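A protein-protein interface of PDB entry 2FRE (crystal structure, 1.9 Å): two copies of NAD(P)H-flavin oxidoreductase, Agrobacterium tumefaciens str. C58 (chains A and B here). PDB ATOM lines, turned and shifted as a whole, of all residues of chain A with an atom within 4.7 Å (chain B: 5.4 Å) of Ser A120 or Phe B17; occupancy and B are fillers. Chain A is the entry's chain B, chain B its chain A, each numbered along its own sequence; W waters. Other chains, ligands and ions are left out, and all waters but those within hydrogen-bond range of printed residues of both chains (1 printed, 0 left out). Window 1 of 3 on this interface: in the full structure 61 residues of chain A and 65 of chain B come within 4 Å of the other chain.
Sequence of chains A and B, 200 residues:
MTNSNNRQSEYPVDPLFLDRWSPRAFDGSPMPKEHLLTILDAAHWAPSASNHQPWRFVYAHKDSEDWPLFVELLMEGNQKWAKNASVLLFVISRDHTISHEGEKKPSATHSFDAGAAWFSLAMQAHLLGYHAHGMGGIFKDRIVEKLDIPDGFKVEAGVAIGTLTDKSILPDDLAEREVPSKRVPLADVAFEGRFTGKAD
Water W1 lies within hydrogen-bond range of O of Phe B17 (2.7 Å), NE of Arg B20 (2.8 Å) and O of Trp A45 (3.4 Å).
Phe A119 touches its own counterpart, Phe B119.
1 position is printed for both chains.
Of the 16 pairs that touch across the chains among the printed residues, 1 has its exchanged pair printed and touching as well.
Of the printed residues of chain B, Ala A46 touches Arg B20 (3.9 Å).
Printed residues of chain B within 4 Å of Ala A116: Phe B119.
Trp A118 touches none of the printed residues of chain B.
Of the printed residues of chain B, Ser A120 touches Phe B17 and Phe B119.
Of the printed residues of chain A, Val B13 touches Ala A42 (3.5 Å) and Gln A124 (3.4 Å).
Of chain A, only Ala A42, Trp A45, Ser A120, Met A123 and Gln A124 come within 4 Å of Phe B17.
The nearest residue of chain A that does not touch Phe B17 is Leu A127 (4.1 Å).
The nearest printed residue of chain B that does not touch Phe A119 is Phe B17 (5.7 Å).
The backbone NH of Asp B14 lies close to the side-chain amide nitrogen of Gln A124, 2.9 Å away.
The backbone carbonyl oxygen of Trp A45 lies within hydrogen-bond range of the guanidinium group of Arg B20 (3.1 Å).
Of the 14 printed residues of chain A, 9 touch a printed residue of chain B.
Hydrophobic or aromatic side chains of chain A within 4 Å of the printed part of chain B: Ala A42, Trp A45, Ala A116, Phe A119, Met A123 and Leu A127.
Of the 10 printed residues of chain B, 7 touch a printed residue of chain A.
Printed residues of chain B that touch a printed residue of chain A: Arg B7, Val B13, Asp B14, Phe B17, Leu B18, Arg B20 and Phe B119.
Among the printed residues, 16 pairs touch across the chains.
The guanidinium group (NH1) of Arg B7 lies within hydrogen-bond range of the backbone carbonyl oxygen (O) of Leu B18, 2.9 Å away.
The backbone carbonyl oxygen of Arg B20 lies within hydrogen-bond range of the guanidinium group of Arg B7 (2.9 Å).
The side-chain carboxylate of Asp B14 sits at hydrogen-bond distance from the backbone NH of Leu B16, 2.9 Å away.
The backbone carbonyl oxygen (O) of Ala A116 sits at hydrogen-bond distance from the side-chain hydroxyl (OG) of Ser A120, at 2.9 Å.
Among the printed residues, pairs that only touch across the chains: Ala A42 with Val B13, Ala A42 with Phe B17, Trp A45 with Arg B7, Trp A45 with Phe B17, Trp A45 with Leu B18, Ala A46 with Arg B20, Ala A116 with Phe B119, Phe A119 with Phe B119, Ser A120 with Phe B17, Ser A120 with Phe B119, Met A123 with Phe B17, Gln A124 with Val B13, Gln A124 with Phe B17 and Leu A127 with Asp B14.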
ATOM      1  N   ALA A  42     -27.249 -27.682 -16.255  1.00  0.00           N
ATOM      2  CA  ALA A  42     -25.995 -27.475 -16.976  1.00  0.00           C
ATOM      3  C   ALA A  42     -25.644 -26.000 -17.016  1.00  0.00           C
ATOM      4  O   ALA A  42     -24.517 -25.643 -16.720  1.00  0.00           O
ATOM      5  CB  ALA A  42     -26.086 -28.046 -18.379  1.00  0.00           C
ATOM      6  N   ALA A  43     -26.615 -25.154 -17.376  1.00  0.00           N
ATOM      7  CA  ALA A  43     -26.424 -23.692 -17.408  1.00  0.00           C
ATOM      8  C   ALA A  43     -25.908 -23.124 -16.089  1.00  0.00           C
ATOM      9  O   ALA A  43     -24.980 -22.276 -16.077  1.00  0.00           O
ATOM     10  CB  ALA A  43     -27.727 -22.985 -17.827  1.00  0.00           C
ATOM     11  N   TRP A  45     -24.178 -24.529 -13.820  1.00  0.00           N
ATOM     12  CA  TRP A  45     -22.800 -24.945 -13.563  1.00  0.00           C
ATOM     13  C   TRP A  45     -21.756 -24.099 -14.267  1.00  0.00           C
ATOM     14  O   TRP A  45     -20.574 -24.345 -14.093  1.00  0.00           O
ATOM     15  CB  TRP A  45     -22.598 -26.449 -13.873  1.00  0.00           C
ATOM     16  CG  TRP A  45     -23.029 -27.290 -12.754  1.00  0.00           C
ATOM     17  CD1 TRP A  45     -24.151 -28.057 -12.686  1.00  0.00           C
ATOM     18  CD2 TRP A  45     -22.346 -27.454 -11.504  1.00  0.00           C
ATOM     19  NE1 TRP A  45     -24.208 -28.695 -11.459  1.00  0.00           N
ATOM     20  CE2 TRP A  45     -23.121 -28.315 -10.712  1.00  0.00           C
ATOM     21  CE3 TRP A  45     -21.165 -26.920 -10.962  1.00  0.00           C
ATOM     22  CZ2 TRP A  45     -22.739 -28.674  -9.415  1.00  0.00           C
ATOM     23  CZ3 TRP A  45     -20.796 -27.284  -9.682  1.00  0.00           C
ATOM     24  CH2 TRP A  45     -21.584 -28.137  -8.924  1.00  0.00           C
ATOM     25  N   ALA A  46     -22.152 -23.056 -14.997  1.00  0.00           N
ATOM     26  CA  ALA A  46     -21.175 -22.183 -15.618  1.00  0.00           C
ATOM     27  C   ALA A  46     -20.242 -21.531 -14.591  1.00  0.00           C
ATOM     28  O   ALA A  46     -20.594 -21.412 -13.416  1.00  0.00           O
ATOM     29  CB  ALA A  46     -21.871 -21.110 -16.432  1.00  0.00           C
ATOM     30  N   ALA A 116     -21.997 -17.099 -20.495  1.00  0.00           N
ATOM     31  CA  ALA A 116     -21.403 -18.428 -20.303  1.00  0.00           C
ATOM     32  C   ALA A 116     -22.480 -19.470 -19.926  1.00  0.00           C
ATOM     33  O   ALA A 116     -22.464 -20.611 -20.395  1.00  0.00           O
ATOM     34  CB  ALA A 116     -20.339 -18.385 -19.254  1.00  0.00           C
ATOM     35  N   ALA A 117     -23.411 -19.053 -19.076  1.00  0.00           N
ATOM     36  CA  ALA A 117     -24.541 -19.893 -18.687  1.00  0.00           C
ATOM     37  C   ALA A 117     -25.419 -20.194 -19.915  1.00  0.00           C
ATOM     38  O   ALA A 117     -25.882 -21.328 -20.098  1.00  0.00           O
ATOM     39  CB  ALA A 117     -25.342 -19.196 -17.601  1.00  0.00           C
ATOM     40  N   TRP A 118     -25.625 -19.184 -20.753  1.00  0.00           N
ATOM     41  CA  TRP A 118     -26.414 -19.366 -21.992  1.00  0.00           C
ATOM     42  C   TRP A 118     -25.737 -20.352 -22.946  1.00  0.00           C
ATOM     43  O   TRP A 118     -26.410 -21.199 -23.499  1.00  0.00           O
ATOM     44  CB  TRP A 118     -26.709 -18.013 -22.663  1.00  0.00           C
ATOM     45  CG  TRP A 118     -26.603 -17.970 -24.159  1.00  0.00           C
ATOM     46  CD1 TRP A 118     -25.687 -17.263 -24.893  1.00  0.00           C
ATOM     47  CD2 TRP A 118     -27.456 -18.626 -25.107  1.00  0.00           C
ATOM     48  NE1 TRP A 118     -25.918 -17.439 -26.236  1.00  0.00           N
ATOM     49  CE2 TRP A 118     -26.980 -18.295 -26.395  1.00  0.00           C
ATOM     50  CE3 TRP A 118     -28.551 -19.498 -24.998  1.00  0.00           C
ATOM     51  CZ2 TRP A 118     -27.592 -18.777 -27.568  1.00  0.00           C
ATOM     52  CZ3 TRP A 118     -29.150 -19.981 -26.162  1.00  0.00           C
ATOM     53  CH2 TRP A 118     -28.674 -19.613 -27.427  1.00  0.00           C
ATOM     54  N   PHE A 119     -24.420 -20.274 -23.154  1.00  0.00           N
ATOM     55  CA  PHE A 119     -23.797 -21.279 -24.026  1.00  0.00           C
ATOM     56  C   PHE A 119     -23.951 -22.677 -23.454  1.00  0.00           C
ATOM     57  O   PHE A 119     -24.234 -23.623 -24.188  1.00  0.00           O
ATOM     58  CB  PHE A 119     -22.325 -21.006 -24.348  1.00  0.00           C
ATOM     59  CG  PHE A 119     -21.783 -21.920 -25.394  1.00  0.00           C
ATOM     60  CD1 PHE A 119     -21.905 -21.617 -26.744  1.00  0.00           C
ATOM     61  CD2 PHE A 119     -21.205 -23.127 -25.035  1.00  0.00           C
ATOM     62  CE1 PHE A 119     -21.428 -22.485 -27.706  1.00  0.00           C
ATOM     63  CE2 PHE A 119     -20.732 -23.989 -25.992  1.00  0.00           C
ATOM     64  CZ  PHE A 119     -20.850 -23.686 -27.320  1.00  0.00           C
ATOM     65  N   SER A 120     -23.738 -22.807 -22.139  1.00  0.00           N
ATOM     66  CA  SER A 120     -23.897 -24.060 -21.442  1.00  0.00           C
ATOM     67  C   SER A 120     -25.316 -24.622 -21.654  1.00  0.00           C
ATOM     68  O   SER A 120     -25.473 -25.799 -21.970  1.00  0.00           O
ATOM     69  CB  SER A 120     -23.603 -23.885 -19.955  1.00  0.00           C
ATOM     70  OG  SER A 120     -22.282 -23.407 -19.732  1.00  0.00           O
ATOM     71  N   LEU A 121     -26.318 -23.750 -21.510  1.00  0.00           N
ATOM     72  CA  LEU A 121     -27.727 -24.072 -21.795  1.00  0.00           C
ATOM     73  C   LEU A 121     -27.879 -24.651 -23.188  1.00  0.00           C
ATOM     74  O   LEU A 121     -28.435 -25.739 -23.379  1.00  0.00           O
ATOM     75  CB  LEU A 121     -28.596 -22.799 -21.644  1.00  0.00           C
ATOM     76  CG  LEU A 121     -30.121 -22.868 -21.683  1.00  0.00           C
ATOM     77  CD1 LEU A 121     -30.702 -21.516 -21.132  1.00  0.00           C
ATOM     78  CD2 LEU A 121     -30.615 -23.148 -23.066  1.00  0.00           C
ATOM     79  N   ALA A 122     -27.402 -23.905 -24.165  1.00  0.00           N
ATOM     80  CA  ALA A 122     -27.461 -24.318 -25.567  1.00  0.00           C
ATOM     81  C   ALA A 122     -26.712 -25.633 -25.869  1.00  0.00           C
ATOM     82  O   ALA A 122     -27.167 -26.440 -26.695  1.00  0.00           O
ATOM     83  CB  ALA A 122     -26.956 -23.192 -26.450  1.00  0.00           C
ATOM     84  N   MET A 123     -25.573 -25.830 -25.226  1.00  0.00           N
ATOM     85  CA  MET A 123     -24.868 -27.069 -25.426  1.00  0.00           C
ATOM     86  C   MET A 123     -25.497 -28.316 -24.830  1.00  0.00           C
ATOM     87  O   MET A 123     -25.543 -29.354 -25.459  1.00  0.00           O
ATOM     88  CB  MET A 123     -23.331 -26.981 -25.390  1.00  0.00           C
ATOM     89  CG  MET A 123     -22.602 -26.797 -24.097  1.00  0.00           C
ATOM     90  SD  MET A 123     -21.035 -28.064 -23.845  1.00  0.00           S
ATOM     91  CE  MET A 123     -19.267 -27.244 -24.525  1.00  0.00           C
ATOM     92  N   GLN A 124     -26.017 -28.178 -23.626  1.00  0.00           N
ATOM     93  CA  GLN A 124     -26.740 -29.279 -22.985  1.00  0.00           C
ATOM     94  C   GLN A 124     -28.031 -29.587 -23.746  1.00  0.00           C
ATOM     95  O   GLN A 124     -28.398 -30.748 -23.895  1.00  0.00           O
ATOM     96  CB  GLN A 124     -27.026 -28.980 -21.517  1.00  0.00           C
ATOM     97  CG  GLN A 124     -27.768 -30.114 -20.770  1.00  0.00           C
ATOM     98  CD  GLN A 124     -27.004 -31.445 -20.775  1.00  0.00           C
ATOM     99  OE1 GLN A 124     -27.134 -32.284 -21.696  1.00  0.00           O
ATOM    100  NE2 GLN A 124     -26.208 -31.632 -19.774  1.00  0.00           N
ATOM    101  N   LEU A 127     -26.894 -31.555 -26.707  1.00  0.00           N
ATOM    102  CA  LEU A 127     -26.530 -32.918 -26.348  1.00  0.00           C
ATOM    103  C   LEU A 127     -27.735 -33.833 -26.066  1.00  0.00           C
ATOM    104  O   LEU A 127     -27.621 -35.053 -26.192  1.00  0.00           O
ATOM    105  CB  LEU A 127     -25.578 -32.923 -25.148  1.00  0.00           C
ATOM    106  CG  LEU A 127     -24.171 -32.398 -25.421  1.00  0.00           C
ATOM    107  CD1 LEU A 127     -23.509 -32.039 -24.076  1.00  0.00           C
ATOM    108  CD2 LEU A 127     -23.337 -33.372 -26.232  1.00  0.00           C
ATOM    109  N   ARG B   7     -18.340 -33.167  -7.528  1.00  0.00           N
ATOM    110  CA  ARG B   7     -19.572 -32.404  -7.661  1.00  0.00           C
ATOM    111  C   ARG B   7     -20.740 -33.328  -7.962  1.00  0.00           C
ATOM    112  O   ARG B   7     -20.589 -34.358  -8.607  1.00  0.00           O
ATOM    113  CB  ARG B   7     -19.474 -31.372  -8.791  1.00  0.00           C
ATOM    114  CG  ARG B   7     -18.480 -30.283  -8.569  1.00  0.00           C
ATOM    115  CD  ARG B   7     -18.140 -29.574  -9.893  1.00  0.00           C
ATOM    116  NE  ARG B   7     -17.561 -28.252  -9.654  1.00  0.00           N
ATOM    117  CZ  ARG B   7     -17.118 -27.424 -10.604  1.00  0.00           C
ATOM    118  NH1 ARG B   7     -17.109 -27.779 -11.883  1.00  0.00           N
ATOM    119  NH2 ARG B   7     -16.674 -26.225 -10.272  1.00  0.00           N
ATOM    120  N   VAL B  13     -27.033 -34.085 -15.923  1.00  0.00           N
ATOM    121  CA  VAL B  13     -26.207 -33.297 -16.812  1.00  0.00           C
ATOM    122  C   VAL B  13     -25.060 -34.128 -17.370  1.00  0.00           C
ATOM    123  O   VAL B  13     -24.611 -35.098 -16.743  1.00  0.00           O
ATOM    124  CB  VAL B  13     -25.593 -32.056 -16.108  1.00  0.00           C
ATOM    125  CG1 VAL B  13     -26.676 -31.111 -15.628  1.00  0.00           C
ATOM    126  CG2 VAL B  13     -24.675 -32.474 -14.938  1.00  0.00           C
ATOM    127  N   ASP B  14     -24.579 -33.725 -18.545  1.00  0.00           N
ATOM    128  CA  ASP B  14     -23.392 -34.324 -19.110  1.00  0.00           C
ATOM    129  C   ASP B  14     -22.272 -34.073 -18.125  1.00  0.00           C
ATOM    130  O   ASP B  14     -22.150 -32.966 -17.615  1.00  0.00           O
ATOM    131  CB  ASP B  14     -23.030 -33.718 -20.458  1.00  0.00           C
ATOM    132  CG  ASP B  14     -21.983 -34.533 -21.190  1.00  0.00           C
ATOM    133  OD1 ASP B  14     -20.835 -34.609 -20.706  1.00  0.00           O
ATOM    134  OD2 ASP B  14     -22.323 -35.113 -22.238  1.00  0.00           O
ATOM    135  N   PRO B  15     -21.463 -35.106 -17.827  1.00  0.00           N
ATOM    136  CA  PRO B  15     -20.379 -34.889 -16.867  1.00  0.00           C
ATOM    137  C   PRO B  15     -19.399 -33.790 -17.248  1.00  0.00           C
ATOM    138  O   PRO B  15     -18.704 -33.257 -16.378  1.00  0.00           O
ATOM    139  CB  PRO B  15     -19.671 -36.248 -16.829  1.00  0.00           C
ATOM    140  CG  PRO B  15     -20.671 -37.220 -17.288  1.00  0.00           C
ATOM    141  CD  PRO B  15     -21.514 -36.506 -18.286  1.00  0.00           C
ATOM    142  N   LEU B  16     -19.328 -33.461 -18.532  1.00  0.00           N
ATOM    143  CA  LEU B  16     -18.484 -32.364 -18.979  1.00  0.00           C
ATOM    144  C   LEU B  16     -18.765 -31.078 -18.198  1.00  0.00           C
ATOM    145  O   LEU B  16     -17.853 -30.310 -17.914  1.00  0.00           O
ATOM    146  CB  LEU B  16     -18.639 -32.131 -20.474  1.00  0.00           C
ATOM    147  CG  LEU B  16     -18.136 -33.242 -21.412  1.00  0.00           C
ATOM    148  CD1 LEU B  16     -18.707 -33.070 -22.815  1.00  0.00           C
ATOM    149  CD2 LEU B  16     -16.618 -33.316 -21.461  1.00  0.00           C
ATOM    150  N   PHE B  17     -20.018 -30.836 -17.839  1.00  0.00           N
ATOM    151  CA  PHE B  17     -20.355 -29.586 -17.130  1.00  0.00           C
ATOM    152  C   PHE B  17     -19.871 -29.552 -15.680  1.00  0.00           C
ATOM    153  O   PHE B  17     -19.657 -28.472 -15.120  1.00  0.00           O
ATOM    154  CB  PHE B  17     -21.862 -29.348 -17.214  1.00  0.00           C
ATOM    155  CG  PHE B  17     -22.324 -29.099 -18.606  1.00  0.00           C
ATOM    156  CD1 PHE B  17     -22.032 -27.893 -19.233  1.00  0.00           C
ATOM    157  CD2 PHE B  17     -23.036 -30.060 -19.297  1.00  0.00           C
ATOM    158  CE1 PHE B  17     -22.445 -27.650 -20.516  1.00  0.00           C
ATOM    159  CE2 PHE B  17     -23.445 -29.816 -20.600  1.00  0.00           C
ATOM    160  CZ  PHE B  17     -23.151 -28.611 -21.195  1.00  0.00           C
ATOM    161  N   LEU B  18     -19.687 -30.722 -15.072  1.00  0.00           N
ATOM    162  CA  LEU B  18     -19.095 -30.825 -13.743  1.00  0.00           C
ATOM    163  C   LEU B  18     -17.564 -30.939 -13.786  1.00  0.00           C
ATOM    164  O   LEU B  18     -16.881 -30.511 -12.849  1.00  0.00           O
ATOM    165  CB  LEU B  18     -19.679 -32.044 -13.013  1.00  0.00           C
ATOM    166  CG  LEU B  18     -21.203 -32.103 -12.908  1.00  0.00           C
ATOM    167  CD1 LEU B  18     -21.634 -33.313 -12.044  1.00  0.00           C
ATOM    168  CD2 LEU B  18     -21.746 -30.847 -12.293  1.00  0.00           C
ATOM    169  N   ASP B  19     -17.045 -31.574 -14.833  1.00  0.00           N
ATOM    170  CA  ASP B  19     -15.600 -31.823 -14.982  1.00  0.00           C
ATOM    171  C   ASP B  19     -14.828 -30.573 -15.346  1.00  0.00           C
ATOM    172  O   ASP B  19     -13.656 -30.462 -14.992  1.00  0.00           O
ATOM    173  CB  ASP B  19     -15.338 -32.924 -16.021  1.00  0.00           C
ATOM    174  CG  ASP B  19     -15.774 -34.272 -15.529  1.00  0.00           C
ATOM    175  OD1 ASP B  19     -15.877 -34.458 -14.302  1.00  0.00           O
ATOM    176  OD2 ASP B  19     -16.015 -35.148 -16.358  1.00  0.00           O
ATOM    177  N   ARG B  20     -15.468 -29.634 -16.045  1.00  0.00           N
ATOM    178  CA  ARG B  20     -14.811 -28.346 -16.311  1.00  0.00           C
ATOM    179  C   ARG B  20     -14.699 -27.532 -15.026  1.00  0.00           C
ATOM    180  O   ARG B  20     -15.703 -27.268 -14.381  1.00  0.00           O
ATOM    181  CB  ARG B  20     -15.585 -27.526 -17.323  1.00  0.00           C
ATOM    182  CG  ARG B  20     -14.971 -26.166 -17.641  1.00  0.00           C
ATOM    183  CD  ARG B  20     -15.988 -25.096 -17.791  1.00  0.00           C
ATOM    184  NE  ARG B  20     -16.888 -24.948 -16.651  1.00  0.00           N
ATOM    185  CZ  ARG B  20     -16.579 -24.371 -15.497  1.00  0.00           C
ATOM    186  NH1 ARG B  20     -15.365 -23.892 -15.270  1.00  0.00           N
ATOM    187  NH2 ARG B  20     -17.503 -24.304 -14.546  1.00  0.00           N
ATOM    188  N   PHE B 119     -17.072 -19.432 -22.578  1.00  0.00           N
ATOM    189  CA  PHE B 119     -17.419 -20.794 -22.138  1.00  0.00           C
ATOM    190  C   PHE B 119     -16.952 -21.806 -23.168  1.00  0.00           C
ATOM    191  O   PHE B 119     -16.438 -22.872 -22.826  1.00  0.00           O
ATOM    192  CB  PHE B 119     -18.898 -21.015 -21.838  1.00  0.00           C
ATOM    193  CG  PHE B 119     -19.135 -22.311 -21.186  1.00  0.00           C
ATOM    194  CD1 PHE B 119     -18.976 -22.446 -19.823  1.00  0.00           C
ATOM    195  CD2 PHE B 119     -19.367 -23.447 -21.947  1.00  0.00           C
ATOM    196  CE1 PHE B 119     -19.110 -23.689 -19.203  1.00  0.00           C
ATOM    197  CE2 PHE B 119     -19.507 -24.680 -21.350  1.00  0.00           C
ATOM    198  CZ  PHE B 119     -19.374 -24.818 -19.985  1.00  0.00           C
HETATM  199  O   HOH W   1     -19.428 -26.214 -16.644  1.00  0.00           O
